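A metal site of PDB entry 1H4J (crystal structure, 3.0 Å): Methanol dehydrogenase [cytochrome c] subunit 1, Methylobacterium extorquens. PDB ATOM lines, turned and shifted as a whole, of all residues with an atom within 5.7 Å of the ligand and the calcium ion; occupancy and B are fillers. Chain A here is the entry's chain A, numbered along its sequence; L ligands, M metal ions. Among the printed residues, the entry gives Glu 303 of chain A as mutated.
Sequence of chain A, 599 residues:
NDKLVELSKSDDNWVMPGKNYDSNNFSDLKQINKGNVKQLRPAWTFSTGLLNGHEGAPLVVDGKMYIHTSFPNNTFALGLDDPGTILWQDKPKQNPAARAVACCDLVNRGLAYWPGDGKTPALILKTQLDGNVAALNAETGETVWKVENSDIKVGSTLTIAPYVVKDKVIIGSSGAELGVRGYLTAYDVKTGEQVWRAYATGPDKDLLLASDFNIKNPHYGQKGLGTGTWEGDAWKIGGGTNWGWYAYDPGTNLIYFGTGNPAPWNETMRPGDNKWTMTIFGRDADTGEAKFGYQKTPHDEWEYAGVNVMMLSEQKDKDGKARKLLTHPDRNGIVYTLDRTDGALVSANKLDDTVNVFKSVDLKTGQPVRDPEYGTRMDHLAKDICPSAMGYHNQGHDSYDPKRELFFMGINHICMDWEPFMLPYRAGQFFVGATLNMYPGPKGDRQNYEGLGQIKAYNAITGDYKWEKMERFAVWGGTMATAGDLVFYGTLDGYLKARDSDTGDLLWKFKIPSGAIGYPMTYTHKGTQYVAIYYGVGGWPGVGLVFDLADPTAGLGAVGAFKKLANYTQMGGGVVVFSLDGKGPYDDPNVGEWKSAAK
O of Thr 159 lies within hydrogen-bond range of N of Arg 109, at 2.8 Å. The backbone carbonyl oxygen (O) of Trp 476 lies close to the side-chain amide oxygen (OE1) of Gln 395 (3.1 Å). The backbone carbonyl oxygen (O) of Trp 243 is in hydrogen-bond range of the guanidinium group (NH1) of Arg 109, at 3.0 Å. NH2 of Arg 331 sits at hydrogen-bond distance from O of Ala 389 (2.9 Å). NH2 of Arg 331 is in salt-bridge range of OE1 of Glu 303, at 3.5 Å. The backbone carbonyl oxygen (O) of Ser 174 is in hydrogen-bond range of the backbone NH (N) of Thr 157 (3.2 Å). OE1 of Glu 55 lies within salt-bridge range of NE of Arg 109, at 3.0 Å. OD2 of Asp 105 lies within hydrogen-bond range of N of Gly 539, at 3.0 Å.
Within 4 Å of the calcium ion: Glu 177, Asn 261 and Glu 303. The nearest printed residue that does not touch the calcium ion is Ala 305 (4.6 Å).
The side-chain hydroxyl (OG1) of Thr 241 is in hydrogen-bond range of an oxygen (O5) of the ligand. NH2 of Arg 109 is in salt-bridge range of O8 of the ligand, at 2.8 Å. N of Trp 540 is in hydrogen-bond range of O2 of the ligand (3.0 Å). The side-chain carboxylate (OE2) of Glu 55 sits close to an oxygen (O1) of the ligand. O7 of the ligand sits at hydrogen-bond distance from OG of Ser 174, 3.2 Å away. O5 of the ligand sits at hydrogen-bond distance from N of Ala 176 (3.3 Å). The guanidinium group (NH1) of Arg 331 is in hydrogen-bond range of an oxygen (O3) of the ligand (3.0 Å). An oxygen (O5) of the ligand lies within hydrogen-bond range of the backbone NH (N) of Gly 175 (3.0 Å). O2 of the ligand sits at hydrogen-bond distance from NE1 of Trp 476, at 2.8 Å. O7 of the ligand sits at hydrogen-bond distance from OG1 of Thr 159. The side-chain amide nitrogen of Asn 394 sits at hydrogen-bond distance from an oxygen (O3) of the ligand.
The calcium ion is bound by a nitrogen (N2) of the ligand (2.3 Å), the side-chain carboxylate (OE2) of Glu 177 (2.4 Å), the side-chain carboxylate (OE2) of Glu 303 (2.4 Å), an oxygen (O6) of the ligand (2.6 Å), an oxygen (O4) of the ligand (2.6 Å), the side-chain carboxylate (OE1) of Glu 177 (2.7 Å) and the side-chain amide oxygen (OD1) of Asn 261 (2.7 Å). The calcium ion has seven donor atoms within binding distance.
Cys 103 touches the ligand. Cys 104 touches the ligand. CG2 of Val 107 touches O1 of the ligand (3.6 Å). Trp 243 touches the ligand. Gly 539 touches the ligand. Pro 541 touches the ligand.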
ATOM      1  N   GLU A  55      14.527  10.205 -11.909  1.00  0.00           N
ATOM      2  CA  GLU A  55      15.984  10.051 -11.915  1.00  0.00           C
ATOM      3  C   GLU A  55      16.563  10.056 -13.329  1.00  0.00           C
ATOM      4  O   GLU A  55      15.852  10.194 -14.322  1.00  0.00           O
ATOM      5  CB  GLU A  55      16.329   8.741 -11.219  1.00  0.00           C
ATOM      6  CG  GLU A  55      15.919   8.738  -9.741  1.00  0.00           C
ATOM      7  CD  GLU A  55      16.370   7.440  -9.095  1.00  0.00           C
ATOM      8  OE1 GLU A  55      16.743   6.528  -9.823  1.00  0.00           O
ATOM      9  OE2 GLU A  55      16.339   7.359  -7.874  1.00  0.00           O
ATOM     10  N   CYS A 103      11.023  -1.735  -4.123  1.00  0.00           N
ATOM     11  CA  CYS A 103      11.564  -1.288  -2.845  1.00  0.00           C
ATOM     12  C   CYS A 103      11.628   0.199  -2.588  1.00  0.00           C
ATOM     13  O   CYS A 103      11.238   0.709  -1.541  1.00  0.00           O
ATOM     14  CB  CYS A 103      13.000  -1.777  -2.657  1.00  0.00           C
ATOM     15  SG  CYS A 103      14.343  -0.892  -3.587  1.00  0.00           S
ATOM     16  N   CYS A 104      12.139   0.875  -3.589  1.00  0.00           N
ATOM     17  CA  CYS A 104      12.462   2.261  -3.445  1.00  0.00           C
ATOM     18  C   CYS A 104      11.869   3.295  -4.399  1.00  0.00           C
ATOM     19  O   CYS A 104      12.608   4.035  -5.041  1.00  0.00           O
ATOM     20  CB  CYS A 104      13.986   2.287  -3.477  1.00  0.00           C
ATOM     21  SG  CYS A 104      14.795   0.854  -2.627  1.00  0.00           S
ATOM     22  N   ASP A 105      10.543   3.354  -4.450  1.00  0.00           N
ATOM     23  CA  ASP A 105       9.833   4.304  -5.321  1.00  0.00           C
ATOM     24  C   ASP A 105       9.890   3.856  -6.775  1.00  0.00           C
ATOM     25  O   ASP A 105      10.816   3.153  -7.184  1.00  0.00           O
ATOM     26  CB  ASP A 105      10.401   5.716  -5.173  1.00  0.00           C
ATOM     27  CG  ASP A 105       9.502   6.778  -5.820  1.00  0.00           C
ATOM     28  OD1 ASP A 105       8.274   6.580  -5.853  1.00  0.00           O
ATOM     29  OD2 ASP A 105      10.035   7.811  -6.277  1.00  0.00           O
ATOM     30  N   VAL A 107      10.972   4.601  -9.732  1.00  0.00           N
ATOM     31  CA  VAL A 107      11.916   5.331 -10.589  1.00  0.00           C
ATOM     32  C   VAL A 107      12.499   4.585 -11.789  1.00  0.00           C
ATOM     33  O   VAL A 107      12.301   3.384 -11.962  1.00  0.00           O
ATOM     34  CB  VAL A 107      13.070   5.894  -9.742  1.00  0.00           C
ATOM     35  CG1 VAL A 107      12.518   6.778  -8.636  1.00  0.00           C
ATOM     36  CG2 VAL A 107      13.870   4.775  -9.147  1.00  0.00           C
ATOM     37  N   ARG A 109      16.217   5.071 -14.272  1.00  0.00           N
ATOM     38  CA  ARG A 109      17.408   5.855 -14.572  1.00  0.00           C
ATOM     39  C   ARG A 109      17.661   6.367 -15.975  1.00  0.00           C
ATOM     40  O   ARG A 109      18.637   7.095 -16.201  1.00  0.00           O
ATOM     41  CB  ARG A 109      18.638   5.132 -14.032  1.00  0.00           C
ATOM     42  CG  ARG A 109      18.909   5.478 -12.575  1.00  0.00           C
ATOM     43  CD  ARG A 109      19.288   4.282 -11.753  1.00  0.00           C
ATOM     44  NE  ARG A 109      18.573   4.297 -10.490  1.00  0.00           N
ATOM     45  CZ  ARG A 109      18.019   3.232  -9.936  1.00  0.00           C
ATOM     46  NH1 ARG A 109      18.092   2.058 -10.554  1.00  0.00           N
ATOM     47  NH2 ARG A 109      17.359   3.344  -8.797  1.00  0.00           N
ATOM     48  N   THR A 157      11.974  -6.551 -10.631  1.00  0.00           N
ATOM     49  CA  THR A 157      11.514  -5.399 -11.388  1.00  0.00           C
ATOM     50  C   THR A 157      12.690  -4.797 -12.144  1.00  0.00           C
ATOM     51  O   THR A 157      13.782  -5.355 -12.139  1.00  0.00           O
ATOM     52  CB  THR A 157      10.915  -4.319 -10.466  1.00  0.00           C
ATOM     53  OG1 THR A 157      11.832  -4.055  -9.384  1.00  0.00           O
ATOM     54  CG2 THR A 157       9.580  -4.778  -9.894  1.00  0.00           C
ATOM     55  N   THR A 159      14.580  -0.868 -13.054  1.00  0.00           N
ATOM     56  CA  THR A 159      14.671   0.580 -12.865  1.00  0.00           C
ATOM     57  C   THR A 159      15.952   1.103 -13.529  1.00  0.00           C
ATOM     58  O   THR A 159      16.086   2.298 -13.784  1.00  0.00           O
ATOM     59  CB  THR A 159      14.714   0.960 -11.374  1.00  0.00           C
ATOM     60  OG1 THR A 159      15.822   0.322 -10.743  1.00  0.00           O
ATOM     61  CG2 THR A 159      13.443   0.514 -10.683  1.00  0.00           C
ATOM     62  N   SER A 173      19.230  -5.627 -13.339  1.00  0.00           N
ATOM     63  CA  SER A 173      18.132  -6.284 -12.650  1.00  0.00           C
ATOM     64  C   SER A 173      17.929  -5.703 -11.246  1.00  0.00           C
ATOM     65  O   SER A 173      18.817  -5.110 -10.645  1.00  0.00           O
ATOM     66  CB  SER A 173      18.443  -7.780 -12.567  1.00  0.00           C
ATOM     67  OG  SER A 173      19.734  -7.970 -11.989  1.00  0.00           O
ATOM     68  N   SER A 174      16.721  -5.816 -10.675  1.00  0.00           N
ATOM     69  CA  SER A 174      16.452  -5.251  -9.354  1.00  0.00           C
ATOM     70  C   SER A 174      15.570  -6.200  -8.563  1.00  0.00           C
ATOM     71  O   SER A 174      14.755  -6.926  -9.159  1.00  0.00           O
ATOM     72  CB  SER A 174      15.729  -3.901  -9.462  1.00  0.00           C
ATOM     73  OG  SER A 174      16.468  -2.957 -10.226  1.00  0.00           O
ATOM     74  N   GLY A 175      15.713  -6.212  -7.237  1.00  0.00           N
ATOM     75  CA  GLY A 175      14.866  -7.076  -6.420  1.00  0.00           C
ATOM     76  C   GLY A 175      15.456  -7.730  -5.190  1.00  0.00           C
ATOM     77  O   GLY A 175      14.750  -8.475  -4.501  1.00  0.00           O
ATOM     78  N   ALA A 176      16.734  -7.473  -4.892  1.00  0.00           N
ATOM     79  CA  ALA A 176      17.377  -8.071  -3.736  1.00  0.00           C
ATOM     80  C   ALA A 176      16.570  -7.925  -2.441  1.00  0.00           C
ATOM     81  O   ALA A 176      16.651  -8.780  -1.568  1.00  0.00           O
ATOM     82  CB  ALA A 176      18.747  -7.478  -3.552  1.00  0.00           C
ATOM     83  N   GLU A 177      15.790  -6.860  -2.320  1.00  0.00           N
ATOM     84  CA  GLU A 177      14.994  -6.713  -1.105  1.00  0.00           C
ATOM     85  C   GLU A 177      13.894  -7.758  -1.047  1.00  0.00           C
ATOM     86  O   GLU A 177      13.180  -7.868  -0.043  1.00  0.00           O
ATOM     87  CB  GLU A 177      14.378  -5.316  -1.005  1.00  0.00           C
ATOM     88  CG  GLU A 177      15.215  -4.322  -0.213  1.00  0.00           C
ATOM     89  CD  GLU A 177      16.543  -4.054  -0.854  1.00  0.00           C
ATOM     90  OE1 GLU A 177      17.474  -4.852  -0.639  1.00  0.00           O
ATOM     91  OE2 GLU A 177      16.662  -3.039  -1.579  1.00  0.00           O
ATOM     92  N   THR A 241      21.734  -8.275  -7.393  1.00  0.00           N
ATOM     93  CA  THR A 241      21.188  -7.562  -8.544  1.00  0.00           C
ATOM     94  C   THR A 241      22.011  -6.322  -8.889  1.00  0.00           C
ATOM     95  O   THR A 241      22.601  -5.718  -8.006  1.00  0.00           O
ATOM     96  CB  THR A 241      19.754  -7.112  -8.264  1.00  0.00           C
ATOM     97  OG1 THR A 241      19.737  -6.337  -7.051  1.00  0.00           O
ATOM     98  CG2 THR A 241      18.822  -8.323  -8.105  1.00  0.00           C
ATOM     99  N   TRP A 243      21.624  -2.680 -10.518  1.00  0.00           N
ATOM    100  CA  TRP A 243      20.735  -1.631 -10.995  1.00  0.00           C
ATOM    101  C   TRP A 243      21.396  -0.262 -11.130  1.00  0.00           C
ATOM    102  O   TRP A 243      20.723   0.740 -11.325  1.00  0.00           O
ATOM    103  CB  TRP A 243      19.529  -1.520 -10.038  1.00  0.00           C
ATOM    104  CG  TRP A 243      19.939  -1.574  -8.585  1.00  0.00           C
ATOM    105  CD1 TRP A 243      20.254  -2.687  -7.844  1.00  0.00           C
ATOM    106  CD2 TRP A 243      20.178  -0.455  -7.710  1.00  0.00           C
ATOM    107  NE1 TRP A 243      20.674  -2.333  -6.594  1.00  0.00           N
ATOM    108  CE2 TRP A 243      20.627  -0.974  -6.480  1.00  0.00           C
ATOM    109  CE3 TRP A 243      20.044   0.937  -7.856  1.00  0.00           C
ATOM    110  CZ2 TRP A 243      20.964  -0.142  -5.404  1.00  0.00           C
ATOM    111  CZ3 TRP A 243      20.368   1.753  -6.782  1.00  0.00           C
ATOM    112  CH2 TRP A 243      20.826   1.217  -5.577  1.00  0.00           C
ATOM    113  N   ASN A 261      23.809  -5.803  -3.026  1.00  0.00           N
ATOM    114  CA  ASN A 261      23.758  -6.438  -1.714  1.00  0.00           C
ATOM    115  C   ASN A 261      23.115  -7.816  -1.748  1.00  0.00           C
ATOM    116  O   ASN A 261      22.193  -8.071  -2.518  1.00  0.00           O
ATOM    117  CB  ASN A 261      22.948  -5.581  -0.740  1.00  0.00           C
ATOM    118  CG  ASN A 261      21.469  -5.521  -1.116  1.00  0.00           C
ATOM    119  OD1 ASN A 261      21.088  -4.832  -2.048  1.00  0.00           O
ATOM    120  ND2 ASN A 261      20.639  -6.262  -0.394  1.00  0.00           N
ATOM    121  N   TRP A 265      18.721  -8.908   4.437  1.00  0.00           N
ATOM    122  CA  TRP A 265      19.530  -7.908   5.125  1.00  0.00           C
ATOM    123  C   TRP A 265      20.043  -8.557   6.391  1.00  0.00           C
ATOM    124  O   TRP A 265      21.092  -8.183   6.925  1.00  0.00           O
ATOM    125  CB  TRP A 265      18.696  -6.671   5.468  1.00  0.00           C
ATOM    126  CG  TRP A 265      18.367  -5.807   4.295  1.00  0.00           C
ATOM    127  CD1 TRP A 265      18.300  -6.188   2.987  1.00  0.00           C
ATOM    128  CD2 TRP A 265      17.994  -4.426   4.327  1.00  0.00           C
ATOM    129  NE1 TRP A 265      17.904  -5.135   2.207  1.00  0.00           N
ATOM    130  CE2 TRP A 265      17.711  -4.039   3.001  1.00  0.00           C
ATOM    131  CE3 TRP A 265      17.871  -3.473   5.350  1.00  0.00           C
ATOM    132  CZ2 TRP A 265      17.296  -2.739   2.670  1.00  0.00           C
ATOM    133  CZ3 TRP A 265      17.460  -2.176   5.011  1.00  0.00           C
ATOM    134  CH2 TRP A 265      17.176  -1.826   3.685  1.00  0.00           C
ATOM    135  N   GLU A 303      23.903  -3.641   4.037  1.00  0.00           N
ATOM    136  CA  GLU A 303      23.218  -3.356   2.786  1.00  0.00           C
ATOM    137  C   GLU A 303      23.971  -2.302   1.953  1.00  0.00           C
ATOM    138  O   GLU A 303      23.402  -1.368   1.405  1.00  0.00           O
ATOM    139  CB  GLU A 303      21.820  -2.850   3.116  1.00  0.00           C
ATOM    140  CG  GLU A 303      20.751  -3.446   2.199  1.00  0.00           C
ATOM    141  CD  GLU A 303      20.190  -2.356   1.317  1.00  0.00           C
ATOM    142  OE1 GLU A 303      19.866  -1.294   1.836  1.00  0.00           O
ATOM    143  OE2 GLU A 303      20.086  -2.578   0.112  1.00  0.00           O
ATOM    144  N   ALA A 305      24.845  -2.021  -0.974  1.00  0.00           N
ATOM    145  CA  ALA A 305      24.715  -2.405  -2.392  1.00  0.00           C
ATOM    146  C   ALA A 305      25.809  -1.741  -3.245  1.00  0.00           C
ATOM    147  O   ALA A 305      25.884  -0.537  -3.393  1.00  0.00           O
ATOM    148  CB  ALA A 305      23.331  -1.963  -2.875  1.00  0.00           C
ATOM    149  N   ARG A 331      28.968   2.386  -1.676  1.00  0.00           N
ATOM    150  CA  ARG A 331      28.016   2.618  -0.598  1.00  0.00           C
ATOM    151  C   ARG A 331      28.685   2.434   0.766  1.00  0.00           C
ATOM    152  O   ARG A 331      28.328   3.118   1.733  1.00  0.00           O
ATOM    153  CB  ARG A 331      26.832   1.644  -0.714  1.00  0.00           C
ATOM    154  CG  ARG A 331      25.804   2.020  -1.752  1.00  0.00           C
ATOM    155  CD  ARG A 331      24.650   2.790  -1.138  1.00  0.00           C
ATOM    156  NE  ARG A 331      23.682   1.910  -0.485  1.00  0.00           N
ATOM    157  CZ  ARG A 331      22.730   1.219  -1.127  1.00  0.00           C
ATOM    158  NH1 ARG A 331      22.601   1.307  -2.448  1.00  0.00           N
ATOM    159  NH2 ARG A 331      21.895   0.448  -0.446  1.00  0.00           N
ATOM    160  N   ALA A 389      22.528   2.172   5.597  1.00  0.00           N
ATOM    161  CA  ALA A 389      22.206   1.365   4.424  1.00  0.00           C
ATOM    162  C   ALA A 389      22.104   2.238   3.189  1.00  0.00           C
ATOM    163  O   ALA A 389      22.326   1.777   2.071  1.00  0.00           O
ATOM    164  CB  ALA A 389      20.915   0.579   4.639  1.00  0.00           C
ATOM    165  N   MET A 390      21.754   3.508   3.373  1.00  0.00           N
ATOM    166  CA  MET A 390      21.655   4.407   2.228  1.00  0.00           C
ATOM    167  C   MET A 390      23.066   4.710   1.723  1.00  0.00           C
ATOM    168  O   MET A 390      23.229   5.246   0.635  1.00  0.00           O
ATOM    169  CB  MET A 390      20.955   5.710   2.629  1.00  0.00           C
ATOM    170  CG  MET A 390      19.537   5.525   3.149  1.00  0.00           C
ATOM    171  SD  MET A 390      18.608   7.082   3.320  1.00  0.00           S
ATOM    172  CE  MET A 390      17.395   6.865   2.043  1.00  0.00           C
ATOM    173  N   ASN A 394      25.131   6.968  -3.038  1.00  0.00           N
ATOM    174  CA  ASN A 394      24.140   6.082  -3.595  1.00  0.00           C
ATOM    175  C   ASN A 394      24.095   6.140  -5.124  1.00  0.00           C
ATOM    176  O   ASN A 394      25.120   6.390  -5.770  1.00  0.00           O
ATOM    177  CB  ASN A 394      22.768   6.424  -2.994  1.00  0.00           C
ATOM    178  CG  ASN A 394      21.874   5.198  -2.856  1.00  0.00           C
ATOM    179  OD1 ASN A 394      21.232   4.782  -3.802  1.00  0.00           O
ATOM    180  ND2 ASN A 394      21.837   4.628  -1.656  1.00  0.00           N
ATOM    181  N   GLN A 395      22.915   5.896  -5.674  1.00  0.00           N
ATOM    182  CA  GLN A 395      22.594   5.819  -7.136  1.00  0.00           C
ATOM    183  C   GLN A 395      23.109   7.046  -7.968  1.00  0.00           C
ATOM    184  O   GLN A 395      23.223   6.998  -9.190  1.00  0.00           O
ATOM    185  CB  GLN A 395      21.080   5.702  -7.273  1.00  0.00           C
ATOM    186  CG  GLN A 395      20.590   6.142  -8.658  1.00  0.00           C
ATOM    187  CD  GLN A 395      19.981   7.520  -8.547  1.00  0.00           C
ATOM    188  OE1 GLN A 395      20.406   8.281  -7.687  1.00  0.00           O
ATOM    189  NE2 GLN A 395      19.086   7.831  -9.335  1.00  0.00           N
ATOM    190  N   TRP A 476      22.025  13.294  -3.552  1.00  0.00           N
ATOM    191  CA  TRP A 476      21.562  12.115  -4.259  1.00  0.00           C
ATOM    192  C   TRP A 476      21.635  11.642  -5.719  1.00  0.00           C
ATOM    193  O   TRP A 476      21.763  10.453  -6.005  1.00  0.00           O
ATOM    194  CB  TRP A 476      20.195  11.785  -3.705  1.00  0.00           C
ATOM    195  CG  TRP A 476      19.723  10.391  -3.764  1.00  0.00           C
ATOM    196  CD1 TRP A 476      18.991   9.807  -4.753  1.00  0.00           C
ATOM    197  CD2 TRP A 476      19.856   9.414  -2.731  1.00  0.00           C
ATOM    198  NE1 TRP A 476      18.638   8.530  -4.392  1.00  0.00           N
ATOM    199  CE2 TRP A 476      19.154   8.263  -3.152  1.00  0.00           C
ATOM    200  CE3 TRP A 476      20.485   9.401  -1.477  1.00  0.00           C
ATOM    201  CZ2 TRP A 476      19.070   7.114  -2.381  1.00  0.00           C
ATOM    202  CZ3 TRP A 476      20.402   8.265  -0.712  1.00  0.00           C
ATOM    203  CH2 TRP A 476      19.703   7.127  -1.160  1.00  0.00           C
ATOM    204  N   GLY A 538      12.038  12.087  -5.067  1.00  0.00           N
ATOM    205  CA  GLY A 538      11.553  10.732  -4.917  1.00  0.00           C
ATOM    206  C   GLY A 538      12.698   9.793  -4.594  1.00  0.00           C
ATOM    207  O   GLY A 538      13.646  10.177  -3.905  1.00  0.00           O
ATOM    208  N   GLY A 539      12.642   8.568  -5.101  1.00  0.00           N
ATOM    209  CA  GLY A 539      13.697   7.626  -4.807  1.00  0.00           C
ATOM    210  C   GLY A 539      13.604   7.250  -3.344  1.00  0.00           C
ATOM    211  O   GLY A 539      12.659   7.608  -2.663  1.00  0.00           O
ATOM    212  N   TRP A 540      14.599   6.549  -2.844  1.00  0.00           N
ATOM    213  CA  TRP A 540      14.562   6.137  -1.457  1.00  0.00           C
ATOM    214  C   TRP A 540      14.407   7.297  -0.467  1.00  0.00           C
ATOM    215  O   TRP A 540      13.576   7.249   0.443  1.00  0.00           O
ATOM    216  CB  TRP A 540      15.807   5.309  -1.102  1.00  0.00           C
ATOM    217  CG  TRP A 540      15.653   4.518   0.156  1.00  0.00           C
ATOM    218  CD1 TRP A 540      14.505   4.354   0.893  1.00  0.00           C
ATOM    219  CD2 TRP A 540      16.662   3.751   0.823  1.00  0.00           C
ATOM    220  NE1 TRP A 540      14.734   3.539   1.976  1.00  0.00           N
ATOM    221  CE2 TRP A 540      16.049   3.153   1.955  1.00  0.00           C
ATOM    222  CE3 TRP A 540      18.023   3.506   0.572  1.00  0.00           C
ATOM    223  CZ2 TRP A 540      16.757   2.317   2.833  1.00  0.00           C
ATOM    224  CZ3 TRP A 540      18.720   2.679   1.451  1.00  0.00           C
ATOM    225  CH2 TRP A 540      18.094   2.095   2.558  1.00  0.00           C
ATOM    226  N   PRO A 541      15.208   8.357  -0.626  1.00  0.00           N
ATOM    227  CA  PRO A 541      15.077   9.477   0.319  1.00  0.00           C
ATOM    228  C   PRO A 541      13.725  10.158   0.345  1.00  0.00           C
ATOM    229  O   PRO A 541      13.327  10.715   1.358  1.00  0.00           O
ATOM    230  CB  PRO A 541      16.209  10.421  -0.099  1.00  0.00           C
ATOM    231  CG  PRO A 541      16.386  10.121  -1.559  1.00  0.00           C
ATOM    232  CD  PRO A 541      16.259   8.623  -1.617  1.00  0.00           C
HETATM  233  N1  LIG L   1      17.069   2.792  -5.322  1.00  0.00           N
HETATM  234  C1  LIG L   1      17.260   4.026  -4.689  1.00  0.00           C
HETATM  235  C2  LIG L   1      16.805   5.304  -5.244  1.00  0.00           C
HETATM  236  O1  LIG L   1      16.216   5.174  -6.396  1.00  0.00           O
HETATM  237  O2  LIG L   1      16.973   6.358  -4.669  1.00  0.00           O
HETATM  238  C3  LIG L   1      17.903   3.783  -3.528  1.00  0.00           C
HETATM  239  C4  LIG L   1      18.124   2.393  -3.440  1.00  0.00           C
HETATM  240  C5  LIG L   1      17.578   1.783  -4.587  1.00  0.00           C
HETATM  241  C6  LIG L   1      18.797   1.578  -2.383  1.00  0.00           C
HETATM  242  O3  LIG L   1      19.746   2.034  -1.890  1.00  0.00           O
HETATM  243  C7  LIG L   1      18.897   0.115  -2.513  1.00  0.00           C
HETATM  244  O4  LIG L   1      19.478  -0.501  -1.571  1.00  0.00           O
HETATM  245  C8  LIG L   1      18.280  -0.501  -3.799  1.00  0.00           C
HETATM  246  N2  LIG L   1      18.430  -1.843  -3.870  1.00  0.00           N
HETATM  247  C9  LIG L   1      17.933  -2.548  -4.966  1.00  0.00           C
HETATM  248  C10 LIG L   1      18.182  -4.043  -4.921  1.00  0.00           C
HETATM  249  O5  LIG L   1      17.961  -4.666  -6.063  1.00  0.00           O
HETATM  250  O6  LIG L   1      18.749  -4.620  -4.014  1.00  0.00           O
HETATM  251  C11 LIG L   1      17.270  -1.891  -6.045  1.00  0.00           C
HETATM  252  C12 LIG L   1      17.095  -0.460  -6.021  1.00  0.00           C
HETATM  253  C13 LIG L   1      16.361   0.124  -7.215  1.00  0.00           C
HETATM  254  O7  LIG L   1      16.045  -0.630  -8.098  1.00  0.00           O
HETATM  255  O8  LIG L   1      16.119   1.259  -7.382  1.00  0.00           O
HETATM  256  C14 LIG L   1      17.600   0.320  -4.862  1.00  0.00           C
HETATM  257 CA    CA M   1      19.003  -3.078  -1.962  1.00  0.00          CA
